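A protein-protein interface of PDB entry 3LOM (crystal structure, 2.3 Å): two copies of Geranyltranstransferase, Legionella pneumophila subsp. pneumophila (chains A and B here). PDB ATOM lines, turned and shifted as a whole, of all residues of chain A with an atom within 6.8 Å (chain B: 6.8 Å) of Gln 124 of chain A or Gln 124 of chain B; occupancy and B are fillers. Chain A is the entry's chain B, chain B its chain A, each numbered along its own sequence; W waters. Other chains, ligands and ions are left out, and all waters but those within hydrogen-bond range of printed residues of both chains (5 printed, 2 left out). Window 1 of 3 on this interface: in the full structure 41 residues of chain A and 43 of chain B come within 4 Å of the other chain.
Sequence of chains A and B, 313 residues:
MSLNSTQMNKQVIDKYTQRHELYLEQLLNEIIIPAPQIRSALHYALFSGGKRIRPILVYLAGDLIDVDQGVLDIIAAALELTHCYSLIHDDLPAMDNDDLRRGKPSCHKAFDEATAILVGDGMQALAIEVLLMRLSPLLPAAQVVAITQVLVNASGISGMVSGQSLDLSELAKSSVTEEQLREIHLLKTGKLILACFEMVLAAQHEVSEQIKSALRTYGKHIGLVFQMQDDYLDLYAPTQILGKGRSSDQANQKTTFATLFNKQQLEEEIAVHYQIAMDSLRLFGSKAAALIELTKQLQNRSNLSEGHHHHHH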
ATOM      1  N   ALA A  78      18.782  -1.858  12.881  1.00  0.00           N
ATOM      2  CA  ALA A  78      18.658  -3.315  13.070  1.00  0.00           C
ATOM      3  C   ALA A  78      19.323  -3.835  14.341  1.00  0.00           C
ATOM      4  O   ALA A  78      18.708  -4.576  15.099  1.00  0.00           O
ATOM      5  CB  ALA A  78      19.222  -4.033  11.889  1.00  0.00           C
ATOM      6  N   LEU A  81      17.723  -2.312  17.567  1.00  0.00           N
ATOM      7  CA  LEU A  81      16.489  -3.065  17.794  1.00  0.00           C
ATOM      8  C   LEU A  81      16.734  -4.443  18.418  1.00  0.00           C
ATOM      9  O   LEU A  81      16.038  -4.835  19.367  1.00  0.00           O
ATOM     10  CB  LEU A  81      15.711  -3.217  16.489  1.00  0.00           C
ATOM     11  CG  LEU A  81      14.864  -2.028  16.031  1.00  0.00           C
ATOM     12  CD1 LEU A  81      14.402  -2.234  14.599  1.00  0.00           C
ATOM     13  CD2 LEU A  81      13.677  -1.833  16.942  1.00  0.00           C
ATOM     14  N   THR A  82      17.730  -5.160  17.884  1.00  0.00           N
ATOM     15  CA  THR A  82      18.124  -6.467  18.403  1.00  0.00           C
ATOM     16  C   THR A  82      18.611  -6.329  19.848  1.00  0.00           C
ATOM     17  O   THR A  82      18.084  -6.973  20.733  1.00  0.00           O
ATOM     18  CB  THR A  82      19.187  -7.137  17.511  1.00  0.00           C
ATOM     19  OG1 THR A  82      18.678  -7.259  16.172  1.00  0.00           O
ATOM     20  CG2 THR A  82      19.537  -8.532  18.043  1.00  0.00           C
ATOM     21  N   TYR A  85      15.730  -5.414  22.225  1.00  0.00           N
ATOM     22  CA  TYR A  85      14.848  -6.574  22.472  1.00  0.00           C
ATOM     23  C   TYR A  85      15.451  -7.442  23.588  1.00  0.00           C
ATOM     24  O   TYR A  85      14.740  -7.866  24.499  1.00  0.00           O
ATOM     25  CB  TYR A  85      14.575  -7.410  21.197  1.00  0.00           C
ATOM     26  CG  TYR A  85      15.103  -8.850  21.233  1.00  0.00           C
ATOM     27  CD1 TYR A  85      14.455  -9.843  21.981  1.00  0.00           C
ATOM     28  CD2 TYR A  85      16.241  -9.215  20.519  1.00  0.00           C
ATOM     29  CE1 TYR A  85      14.941 -11.144  22.038  1.00  0.00           C
ATOM     30  CE2 TYR A  85      16.736 -10.522  20.567  1.00  0.00           C
ATOM     31  CZ  TYR A  85      16.074 -11.477  21.328  1.00  0.00           C
ATOM     32  OH  TYR A  85      16.534 -12.773  21.383  1.00  0.00           O
ATOM     33  N   HIS A  89      13.882  -8.465  27.462  1.00  0.00           N
ATOM     34  CA  HIS A  89      13.808  -9.851  27.900  1.00  0.00           C
ATOM     35  C   HIS A  89      14.702 -10.140  29.108  1.00  0.00           C
ATOM     36  O   HIS A  89      14.257 -10.789  30.046  1.00  0.00           O
ATOM     37  CB  HIS A  89      14.062 -10.791  26.734  1.00  0.00           C
ATOM     38  CG  HIS A  89      12.862 -10.973  25.864  1.00  0.00           C
ATOM     39  ND1 HIS A  89      12.821 -11.881  24.830  1.00  0.00           N
ATOM     40  CD2 HIS A  89      11.644 -10.378  25.892  1.00  0.00           C
ATOM     41  CE1 HIS A  89      11.632 -11.833  24.253  1.00  0.00           C
ATOM     42  NE2 HIS A  89      10.899 -10.931  24.879  1.00  0.00           N
ATOM     43  N   VAL A 119       6.764  -7.413  22.881  1.00  0.00           N
ATOM     44  CA  VAL A 119       7.556  -6.331  22.290  1.00  0.00           C
ATOM     45  C   VAL A 119       8.982  -6.774  21.958  1.00  0.00           C
ATOM     46  O   VAL A 119       9.457  -6.536  20.838  1.00  0.00           O
ATOM     47  CB  VAL A 119       7.509  -5.033  23.143  1.00  0.00           C
ATOM     48  CG1 VAL A 119       8.596  -4.050  22.746  1.00  0.00           C
ATOM     49  CG2 VAL A 119       6.166  -4.377  22.959  1.00  0.00           C
ATOM     50  N   GLY A 120       9.636  -7.449  22.906  1.00  0.00           N
ATOM     51  CA  GLY A 120      10.936  -8.089  22.649  1.00  0.00           C
ATOM     52  C   GLY A 120      10.892  -9.001  21.429  1.00  0.00           C
ATOM     53  O   GLY A 120      11.739  -8.911  20.540  1.00  0.00           O
ATOM     54  N   ASP A 121       9.878  -9.857  21.375  1.00  0.00           N
ATOM     55  CA  ASP A 121       9.668 -10.744  20.231  1.00  0.00           C
ATOM     56  C   ASP A 121       9.522  -9.983  18.921  1.00  0.00           C
ATOM     57  O   ASP A 121      10.109 -10.364  17.907  1.00  0.00           O
ATOM     58  CB  ASP A 121       8.428 -11.612  20.460  1.00  0.00           C
ATOM     59  CG  ASP A 121       8.621 -12.638  21.551  1.00  0.00           C
ATOM     60  OD1 ASP A 121       9.757 -12.770  22.051  1.00  0.00           O
ATOM     61  OD2 ASP A 121       7.629 -13.313  21.903  1.00  0.00           O
ATOM     62  N   GLY A 122       8.738  -8.903  18.960  1.00  0.00           N
ATOM     63  CA  GLY A 122       8.458  -8.077  17.783  1.00  0.00           C
ATOM     64  C   GLY A 122       9.638  -7.268  17.280  1.00  0.00           C
ATOM     65  O   GLY A 122       9.816  -7.137  16.069  1.00  0.00           O
ATOM     66  N   MET A 123      10.450  -6.730  18.196  1.00  0.00           N
ATOM     67  CA  MET A 123      11.652  -5.962  17.816  1.00  0.00           C
ATOM     68  C   MET A 123      12.718  -6.847  17.182  1.00  0.00           C
ATOM     69  O   MET A 123      13.485  -6.372  16.331  1.00  0.00           O
ATOM     70  CB  MET A 123      12.274  -5.216  19.005  1.00  0.00           C
ATOM     71  CG  MET A 123      11.347  -4.252  19.705  1.00  0.00           C
ATOM     72  SD  MET A 123      12.046  -3.538  21.205  1.00  0.00           S
ATOM     73  CE  MET A 123      13.006  -2.236  20.531  1.00  0.00           C
ATOM     74  N   GLN A 124      12.792  -8.113  17.618  1.00  0.00           N
ATOM     75  CA  GLN A 124      13.728  -9.058  16.999  1.00  0.00           C
ATOM     76  C   GLN A 124      13.330  -9.288  15.535  1.00  0.00           C
ATOM     77  O   GLN A 124      14.179  -9.208  14.648  1.00  0.00           O
ATOM     78  CB  GLN A 124      13.868 -10.394  17.770  1.00  0.00           C
ATOM     79  CG  GLN A 124      14.700 -11.398  16.965  1.00  0.00           C
ATOM     80  CD  GLN A 124      15.111 -12.688  17.666  1.00  0.00           C
ATOM     81  OE1 GLN A 124      16.195 -13.194  17.395  1.00  0.00           O
ATOM     82  NE2 GLN A 124      14.251 -13.244  18.519  1.00  0.00           N
ATOM     83  N   ALA A 125      12.041  -9.550  15.301  1.00  0.00           N
ATOM     84  CA  ALA A 125      11.483  -9.661  13.944  1.00  0.00           C
ATOM     85  C   ALA A 125      11.605  -8.376  13.132  1.00  0.00           C
ATOM     86  O   ALA A 125      11.989  -8.424  11.960  1.00  0.00           O
ATOM     87  CB  ALA A 125      10.028 -10.109  13.988  1.00  0.00           C
ATOM     88  N   LEU A 126      11.279  -7.240  13.755  1.00  0.00           N
ATOM     89  CA  LEU A 126      11.337  -5.929  13.092  1.00  0.00           C
ATOM     90  C   LEU A 126      12.726  -5.641  12.558  1.00  0.00           C
ATOM     91  O   LEU A 126      12.861  -5.125  11.446  1.00  0.00           O
ATOM     92  CB  LEU A 126      10.893  -4.778  14.021  1.00  0.00           C
ATOM     93  CG  LEU A 126      10.807  -3.377  13.375  1.00  0.00           C
ATOM     94  CD1 LEU A 126       9.855  -3.368  12.172  1.00  0.00           C
ATOM     95  CD2 LEU A 126      10.428  -2.285  14.370  1.00  0.00           C
ATOM     96  N   ALA A 127      13.751  -6.007  13.328  1.00  0.00           N
ATOM     97  CA  ALA A 127      15.142  -5.791  12.919  1.00  0.00           C
ATOM     98  C   ALA A 127      15.483  -6.535  11.622  1.00  0.00           C
ATOM     99  O   ALA A 127      16.264  -6.047  10.801  1.00  0.00           O
ATOM    100  CB  ALA A 127      16.082  -6.194  14.021  1.00  0.00           C
ATOM    101  N   ILE A 128      14.867  -7.701  11.440  1.00  0.00           N
ATOM    102  CA  ILE A 128      15.048  -8.498  10.231  1.00  0.00           C
ATOM    103  C   ILE A 128      14.252  -7.866   9.089  1.00  0.00           C
ATOM    104  O   ILE A 128      14.772  -7.718   7.982  1.00  0.00           O
ATOM    105  CB  ILE A 128      14.628  -9.989  10.440  1.00  0.00           C
ATOM    106  CG1 ILE A 128      15.298 -10.598  11.688  1.00  0.00           C
ATOM    107  CG2 ILE A 128      14.871 -10.828   9.182  1.00  0.00           C
ATOM    108  CD1 ILE A 128      16.809 -10.465  11.752  1.00  0.00           C
ATOM    109  N   GLU A 129      13.003  -7.486   9.374  1.00  0.00           N
ATOM    110  CA  GLU A 129      12.146  -6.779   8.414  1.00  0.00           C
ATOM    111  C   GLU A 129      12.832  -5.553   7.829  1.00  0.00           C
ATOM    112  O   GLU A 129      12.847  -5.380   6.616  1.00  0.00           O
ATOM    113  CB  GLU A 129      10.824  -6.368   9.065  1.00  0.00           C
ATOM    114  CG  GLU A 129       9.818  -5.739   8.105  1.00  0.00           C
ATOM    115  CD  GLU A 129       8.477  -5.454   8.757  1.00  0.00           C
ATOM    116  OE1 GLU A 129       7.934  -4.349   8.532  1.00  0.00           O
ATOM    117  OE2 GLU A 129       7.963  -6.330   9.492  1.00  0.00           O
ATOM    118  N   LEU A 151      23.734 -10.895  11.684  1.00  0.00           N
ATOM    119  CA  LEU A 151      22.903 -10.521  12.830  1.00  0.00           C
ATOM    120  C   LEU A 151      22.301 -11.732  13.518  1.00  0.00           C
ATOM    121  O   LEU A 151      22.397 -11.898  14.735  1.00  0.00           O
ATOM    122  CB  LEU A 151      21.755  -9.599  12.393  1.00  0.00           C
ATOM    123  CG  LEU A 151      20.839  -9.122  13.525  1.00  0.00           C
ATOM    124  CD1 LEU A 151      21.630  -8.288  14.539  1.00  0.00           C
ATOM    125  CD2 LEU A 151      19.682  -8.324  12.969  1.00  0.00           C
ATOM    126  N   VAL A 152      21.665 -12.566  12.716  1.00  0.00           N
ATOM    127  CA  VAL A 152      20.965 -13.732  13.209  1.00  0.00           C
ATOM    128  C   VAL A 152      21.919 -14.825  13.774  1.00  0.00           C
ATOM    129  O   VAL A 152      21.560 -15.543  14.724  1.00  0.00           O
ATOM    130  CB  VAL A 152      19.960 -14.199  12.129  1.00  0.00           C
ATOM    131  CG1 VAL A 152      19.949 -15.659  11.980  1.00  0.00           C
ATOM    132  CG2 VAL A 152      18.568 -13.698  12.475  1.00  0.00           C
ATOM    133  N   SER A 155      23.047 -13.294  17.268  1.00  0.00           N
ATOM    134  CA  SER A 155      21.960 -13.060  18.224  1.00  0.00           C
ATOM    135  C   SER A 155      21.264 -14.341  18.660  1.00  0.00           C
ATOM    136  O   SER A 155      20.534 -14.349  19.656  1.00  0.00           O
ATOM    137  CB  SER A 155      20.910 -12.125  17.620  1.00  0.00           C
ATOM    138  OG  SER A 155      20.059 -12.862  16.761  1.00  0.00           O
ATOM    139  N   GLY A 156      21.466 -15.414  17.905  1.00  0.00           N
ATOM    140  CA  GLY A 156      20.717 -16.646  18.132  1.00  0.00           C
ATOM    141  C   GLY A 156      21.351 -17.624  19.110  1.00  0.00           C
ATOM    142  O   GLY A 156      22.131 -17.229  19.991  1.00  0.00           O
ATOM    143  N   VAL A 161      21.804 -15.953  22.620  1.00  0.00           N
ATOM    144  CA  VAL A 161      20.860 -16.787  23.369  1.00  0.00           C
ATOM    145  C   VAL A 161      21.568 -17.805  24.295  1.00  0.00           C
ATOM    146  O   VAL A 161      21.264 -17.863  25.489  1.00  0.00           O
ATOM    147  CB  VAL A 161      19.769 -17.388  22.467  1.00  0.00           C
ATOM    148  CG1 VAL A 161      19.072 -18.552  23.133  1.00  0.00           C
ATOM    149  CG2 VAL A 161      18.747 -16.302  22.113  1.00  0.00           C
ATOM    150  N   ALA B  78      11.538 -23.685   9.006  1.00  0.00           N
ATOM    151  CA  ALA B  78      11.451 -22.287   9.424  1.00  0.00           C
ATOM    152  C   ALA B  78      10.069 -21.917   9.946  1.00  0.00           C
ATOM    153  O   ALA B  78       9.947 -21.212  10.948  1.00  0.00           O
ATOM    154  CB  ALA B  78      11.834 -21.392   8.288  1.00  0.00           C
ATOM    155  N   LEU B  81       9.590 -23.787  13.361  1.00  0.00           N
ATOM    156  CA  LEU B  81      10.417 -23.083  14.342  1.00  0.00           C
ATOM    157  C   LEU B  81       9.754 -21.789  14.821  1.00  0.00           C
ATOM    158  O   LEU B  81       9.719 -21.527  16.031  1.00  0.00           O
ATOM    159  CB  LEU B  81      11.820 -22.795  13.787  1.00  0.00           C
ATOM    160  CG  LEU B  81      12.847 -23.933  13.760  1.00  0.00           C
ATOM    161  CD1 LEU B  81      13.984 -23.593  12.814  1.00  0.00           C
ATOM    162  CD2 LEU B  81      13.385 -24.218  15.150  1.00  0.00           C
ATOM    163  N   THR B  82       9.218 -21.003  13.878  1.00  0.00           N
ATOM    164  CA  THR B  82       8.469 -19.773  14.207  1.00  0.00           C
ATOM    165  C   THR B  82       7.209 -20.099  15.015  1.00  0.00           C
ATOM    166  O   THR B  82       7.011 -19.545  16.088  1.00  0.00           O
ATOM    167  CB  THR B  82       8.123 -18.919  12.949  1.00  0.00           C
ATOM    168  OG1 THR B  82       9.326 -18.598  12.232  1.00  0.00           O
ATOM    169  CG2 THR B  82       7.429 -17.611  13.355  1.00  0.00           C
ATOM    170  N   TYR B  85       8.274 -21.390  18.633  1.00  0.00           N
ATOM    171  CA  TYR B  85       8.673 -20.253  19.481  1.00  0.00           C
ATOM    172  C   TYR B  85       7.459 -19.525  20.066  1.00  0.00           C
ATOM    173  O   TYR B  85       7.401 -19.277  21.276  1.00  0.00           O
ATOM    174  CB  TYR B  85       9.623 -19.285  18.739  1.00  0.00           C
ATOM    175  CG  TYR B  85       9.152 -17.835  18.625  1.00  0.00           C
ATOM    176  CD1 TYR B  85       9.083 -16.990  19.741  1.00  0.00           C
ATOM    177  CD2 TYR B  85       8.780 -17.313  17.390  1.00  0.00           C
ATOM    178  CE1 TYR B  85       8.634 -15.679  19.621  1.00  0.00           C
ATOM    179  CE2 TYR B  85       8.341 -16.009  17.258  1.00  0.00           C
ATOM    180  CZ  TYR B  85       8.273 -15.196  18.370  1.00  0.00           C
ATOM    181  OH  TYR B  85       7.834 -13.901  18.226  1.00  0.00           O
ATOM    182  N   HIS B  89       6.303 -19.163  24.112  1.00  0.00           N
ATOM    183  CA  HIS B  89       6.104 -17.857  24.735  1.00  0.00           C
ATOM    184  C   HIS B  89       4.677 -17.633  25.214  1.00  0.00           C
ATOM    185  O   HIS B  89       4.477 -17.094  26.304  1.00  0.00           O
ATOM    186  CB  HIS B  89       6.592 -16.727  23.826  1.00  0.00           C
ATOM    187  CG  HIS B  89       8.078 -16.561  23.842  1.00  0.00           C
ATOM    188  ND1 HIS B  89       8.708 -15.425  23.383  1.00  0.00           N
ATOM    189  CD2 HIS B  89       9.059 -17.377  24.299  1.00  0.00           C
ATOM    190  CE1 HIS B  89      10.014 -15.557  23.539  1.00  0.00           C
ATOM    191  NE2 HIS B  89      10.253 -16.732  24.091  1.00  0.00           N
ATOM    192  N   VAL B 119      14.800 -19.971  24.679  1.00  0.00           N
ATOM    193  CA  VAL B 119      14.684 -20.963  23.617  1.00  0.00           C
ATOM    194  C   VAL B 119      13.733 -20.456  22.544  1.00  0.00           C
ATOM    195  O   VAL B 119      14.044 -20.553  21.345  1.00  0.00           O
ATOM    196  CB  VAL B 119      14.311 -22.369  24.183  1.00  0.00           C
ATOM    197  CG1 VAL B 119      13.369 -23.145  23.281  1.00  0.00           C
ATOM    198  CG2 VAL B 119      15.574 -23.159  24.426  1.00  0.00           C
ATOM    199  N   GLY B 120      12.606 -19.887  22.983  1.00  0.00           N
ATOM    200  CA  GLY B 120      11.695 -19.149  22.097  1.00  0.00           C
ATOM    201  C   GLY B 120      12.448 -18.099  21.291  1.00  0.00           C
ATOM    202  O   GLY B 120      12.406 -18.109  20.059  1.00  0.00           O
ATOM    203  N   ASP B 121      13.186 -17.231  21.987  1.00  0.00           N
ATOM    204  CA  ASP B 121      14.009 -16.205  21.338  1.00  0.00           C
ATOM    205  C   ASP B 121      14.966 -16.777  20.301  1.00  0.00           C
ATOM    206  O   ASP B 121      15.082 -16.233  19.209  1.00  0.00           O
ATOM    207  CB  ASP B 121      14.813 -15.423  22.377  1.00  0.00           C
ATOM    208  CG  ASP B 121      13.967 -14.452  23.158  1.00  0.00           C
ATOM    209  OD1 ASP B 121      12.752 -14.357  22.881  1.00  0.00           O
ATOM    210  OD2 ASP B 121      14.524 -13.779  24.052  1.00  0.00           O
ATOM    211  N   GLY B 122      15.652 -17.868  20.652  1.00  0.00           N
ATOM    212  CA  GLY B 122      16.590 -18.527  19.741  1.00  0.00           C
ATOM    213  C   GLY B 122      15.939 -19.224  18.560  1.00  0.00           C
ATOM    214  O   GLY B 122      16.499 -19.222  17.461  1.00  0.00           O
ATOM    215  N   MET B 123      14.765 -19.824  18.779  1.00  0.00           N
ATOM    216  CA  MET B 123      14.001 -20.449  17.693  1.00  0.00           C
ATOM    217  C   MET B 123      13.608 -19.426  16.626  1.00  0.00           C
ATOM    218  O   MET B 123      13.753 -19.702  15.430  1.00  0.00           O
ATOM    219  CB  MET B 123      12.749 -21.169  18.205  1.00  0.00           C
ATOM    220  CG  MET B 123      12.975 -22.568  18.744  1.00  0.00           C
ATOM    221  SD  MET B 123      11.431 -23.415  19.133  1.00  0.00           S
ATOM    222  CE  MET B 123      12.088 -24.796  20.047  1.00  0.00           C
ATOM    223  N   GLN B 124      13.131 -18.252  17.060  1.00  0.00           N
ATOM    224  CA  GLN B 124      12.774 -17.176  16.132  1.00  0.00           C
ATOM    225  C   GLN B 124      13.953 -16.830  15.238  1.00  0.00           C
ATOM    226  O   GLN B 124      13.812 -16.811  14.015  1.00  0.00           O
ATOM    227  CB  GLN B 124      12.238 -15.914  16.845  1.00  0.00           C
ATOM    228  CG  GLN B 124      12.154 -14.685  15.898  1.00  0.00           C
ATOM    229  CD  GLN B 124      11.165 -13.598  16.310  1.00  0.00           C
ATOM    230  OE1 GLN B 124      10.443 -13.069  15.459  1.00  0.00           O
ATOM    231  NE2 GLN B 124      11.139 -13.243  17.602  1.00  0.00           N
ATOM    232  N   ALA B 125      15.110 -16.585  15.854  1.00  0.00           N
ATOM    233  CA  ALA B 125      16.342 -16.341  15.114  1.00  0.00           C
ATOM    234  C   ALA B 125      16.758 -17.529  14.229  1.00  0.00           C
ATOM    235  O   ALA B 125      17.249 -17.318  13.117  1.00  0.00           O
ATOM    236  CB  ALA B 125      17.462 -15.961  16.058  1.00  0.00           C
ATOM    237  N   LEU B 126      16.550 -18.761  14.710  1.00  0.00           N
ATOM    238  CA  LEU B 126      16.971 -19.954  13.958  1.00  0.00           C
ATOM    239  C   LEU B 126      16.210 -20.113  12.648  1.00  0.00           C
ATOM    240  O   LEU B 126      16.821 -20.372  11.610  1.00  0.00           O
ATOM    241  CB  LEU B 126      16.891 -21.248  14.787  1.00  0.00           C
ATOM    242  CG  LEU B 126      17.453 -22.503  14.080  1.00  0.00           C
ATOM    243  CD1 LEU B 126      18.925 -22.332  13.682  1.00  0.00           C
ATOM    244  CD2 LEU B 126      17.250 -23.788  14.880  1.00  0.00           C
ATOM    245  N   ALA B 127      14.890 -19.939  12.713  1.00  0.00           N
ATOM    246  CA  ALA B 127      14.010 -19.963  11.544  1.00  0.00           C
ATOM    247  C   ALA B 127      14.542 -19.096  10.408  1.00  0.00           C
ATOM    248  O   ALA B 127      14.533 -19.514   9.252  1.00  0.00           O
ATOM    249  CB  ALA B 127      12.630 -19.513  11.935  1.00  0.00           C
ATOM    250  N   ILE B 128      15.031 -17.909  10.761  1.00  0.00           N
ATOM    251  CA  ILE B 128      15.627 -16.970   9.814  1.00  0.00           C
ATOM    252  C   ILE B 128      17.022 -17.419   9.350  1.00  0.00           C
ATOM    253  O   ILE B 128      17.322 -17.324   8.158  1.00  0.00           O
ATOM    254  CB  ILE B 128      15.631 -15.538  10.402  1.00  0.00           C
ATOM    255  CG1 ILE B 128      14.191 -15.097  10.670  1.00  0.00           C
ATOM    256  CG2 ILE B 128      16.317 -14.540   9.474  1.00  0.00           C
ATOM    257  CD1 ILE B 128      14.052 -14.164  11.849  1.00  0.00           C
ATOM    258  N   GLU B 129      17.855 -17.919  10.275  1.00  0.00           N
ATOM    259  CA  GLU B 129      19.178 -18.494   9.933  1.00  0.00           C
ATOM    260  C   GLU B 129      19.066 -19.630   8.919  1.00  0.00           C
ATOM    261  O   GLU B 129      19.756 -19.627   7.903  1.00  0.00           O
ATOM    262  CB  GLU B 129      19.919 -18.985  11.189  1.00  0.00           C
ATOM    263  CG  GLU B 129      21.372 -19.437  10.951  1.00  0.00           C
ATOM    264  CD  GLU B 129      22.266 -19.314  12.186  1.00  0.00           C
ATOM    265  OE1 GLU B 129      23.506 -19.297  12.018  1.00  0.00           O
ATOM    266  OE2 GLU B 129      21.751 -19.223  13.318  1.00  0.00           O
ATOM    267  N   LEU B 151       7.676 -14.428   6.097  1.00  0.00           N
ATOM    268  CA  LEU B 151       7.621 -14.989   7.452  1.00  0.00           C
ATOM    269  C   LEU B 151       7.730 -13.914   8.522  1.00  0.00           C
ATOM    270  O   LEU B 151       6.993 -13.914   9.503  1.00  0.00           O
ATOM    271  CB  LEU B 151       8.744 -16.022   7.659  1.00  0.00           C
ATOM    272  CG  LEU B 151       8.807 -16.798   8.983  1.00  0.00           C
ATOM    273  CD1 LEU B 151       7.589 -17.696   9.182  1.00  0.00           C
ATOM    274  CD2 LEU B 151      10.070 -17.634   9.033  1.00  0.00           C
ATOM    275  N   VAL B 152       8.666 -13.004   8.308  1.00  0.00           N
ATOM    276  CA  VAL B 152       8.969 -11.942   9.239  1.00  0.00           C
ATOM    277  C   VAL B 152       7.874 -10.833   9.284  1.00  0.00           C
ATOM    278  O   VAL B 152       7.631 -10.235  10.342  1.00  0.00           O
ATOM    279  CB  VAL B 152      10.419 -11.456   8.959  1.00  0.00           C
ATOM    280  CG1 VAL B 152      10.536  -9.975   8.922  1.00  0.00           C
ATOM    281  CG2 VAL B 152      11.377 -12.059   9.991  1.00  0.00           C
ATOM    282  N   SER B 155       4.972 -12.681  11.221  1.00  0.00           N
ATOM    283  CA  SER B 155       5.303 -13.064  12.597  1.00  0.00           C
ATOM    284  C   SER B 155       5.505 -11.857  13.505  1.00  0.00           C
ATOM    285  O   SER B 155       5.425 -11.966  14.732  1.00  0.00           O
ATOM    286  CB  SER B 155       6.569 -13.924  12.627  1.00  0.00           C
ATOM    287  OG  SER B 155       7.701 -13.125  12.336  1.00  0.00           O
ATOM    288  N   GLY B 156       5.774 -10.709  12.896  1.00  0.00           N
ATOM    289  CA  GLY B 156       6.146  -9.527  13.651  1.00  0.00           C
ATOM    290  C   GLY B 156       4.992  -8.699  14.181  1.00  0.00           C
ATOM    291  O   GLY B 156       3.881  -9.204  14.388  1.00  0.00           O
ATOM    292  N   VAL B 161       2.478 -10.765  16.562  1.00  0.00           N
ATOM    293  CA  VAL B 161       2.752 -10.120  17.848  1.00  0.00           C
ATOM    294  C   VAL B 161       1.615  -9.180  18.301  1.00  0.00           C
ATOM    295  O   VAL B 161       1.233  -9.189  19.485  1.00  0.00           O
ATOM    296  CB  VAL B 161       4.145  -9.417  17.828  1.00  0.00           C
ATOM    297  CG1 VAL B 161       4.265  -8.357  18.915  1.00  0.00           C
ATOM    298  CG2 VAL B 161       5.271 -10.477  17.956  1.00  0.00           C
HETATM  299  O   HOH W   1      17.143 -13.431  24.117  1.00  0.00           O
HETATM  300  O   HOH W   2       5.233  -7.890  11.006  1.00  0.00           O
HETATM  301  O   HOH W   3       5.390 -13.839  20.302  1.00  0.00           O
HETATM  302  O   HOH W   4      12.112 -13.506  20.218  1.00  0.00           O
HETATM  303  O   HOH W   5      22.990 -18.207  16.401  1.00  0.00           O
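Gln 124 of chain A touches just these residues of chain B: Asp 121, Gln 124 and Ala 125. Of chain A, only Asp 121, Gln 124 and Ala 125 come within 4 Å of Gln 124 of chain B. Of the printed residues of chain A, Ala 125 of chain B touches Gln 124, Val 152 and Gly 156. Printed residues of chain A within 4 Å of His 89 of chain B: Asp 121 (2.8 Å). The nearest residue of chain B that does not touch Gln 124 of chain A is Gly 122 of chain B (5.3 Å).
His 89 of chain A touches Asp 121 of chain B, and with the chains exchanged Asp 121 of chain A touches His 89 of chain B. Ile 128 of chain A touches Val 152 of chain B, and with the chains exchanged Val 152 of chain A touches Ile 128 of chain B.
Printed residues of chain B that touch a printed residue of chain A: Tyr 85, His 89, Asp 121, Gly 122, Gln 124, Ala 125, Ile 128, Glu 129, Val 152, Gly 156 and Val 161. Hydrophobic or aromatic side chains of chain B within 4 Å of the printed part of chain A: Tyr 85, His 89, Ala 125, Ile 128, Val 152 and Val 161. Along chain A the printed residues that touch a printed residue of chain B span positions 85 to 161. Among the printed residues, 21 pairs touch across the chains.
ND1 of His 89 of chain B sits at hydrogen-bond distance from OD2 of Asp 121 of chain A (2.8 Å). The side-chain carboxylate (OD2) of Asp 121 of chain B lies close to the side-chain hydroxyl (OH) of Tyr 85 of chain A (3.5 Å). The side-chain carboxylate (OD2) of Asp 121 of chain B is in hydrogen-bond range of a ring nitrogen (ND1) of His 89 of chain A. O of Asp 121 of chain B lies within hydrogen-bond range of NE2 of Gln 124 of chain A (3.2 Å). The backbone carbonyl oxygen of Asp 121 of chain A is in hydrogen-bond range of the side-chain amide nitrogen of Gln 124 of chain B, 3.1 Å away. NE2 of Gln 124 of chain A sits close to NE2 of Gln 124 of chain B, at 3.2 Å. The side-chain carboxylate of Asp 121 of chain A sits close to the side-chain carboxylate of Asp 121 of chain B.
Water W3 lies within hydrogen-bond range of OD2 of Asp 121 of chain A and OH of Tyr 85 of chain B. Water W5 bridges O of Val 152 of chain A (3.5 Å) and OE2 of Glu 129 of chain B (3.5 Å).
The backbone NH (N) of Val 161 of chain B is in hydrogen-bond range of the backbone carbonyl oxygen (O) of Gly 156 of chain B. O of Gly 156 of chain A sits at hydrogen-bond distance from N of Val 161 of chain A (2.9 Å).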
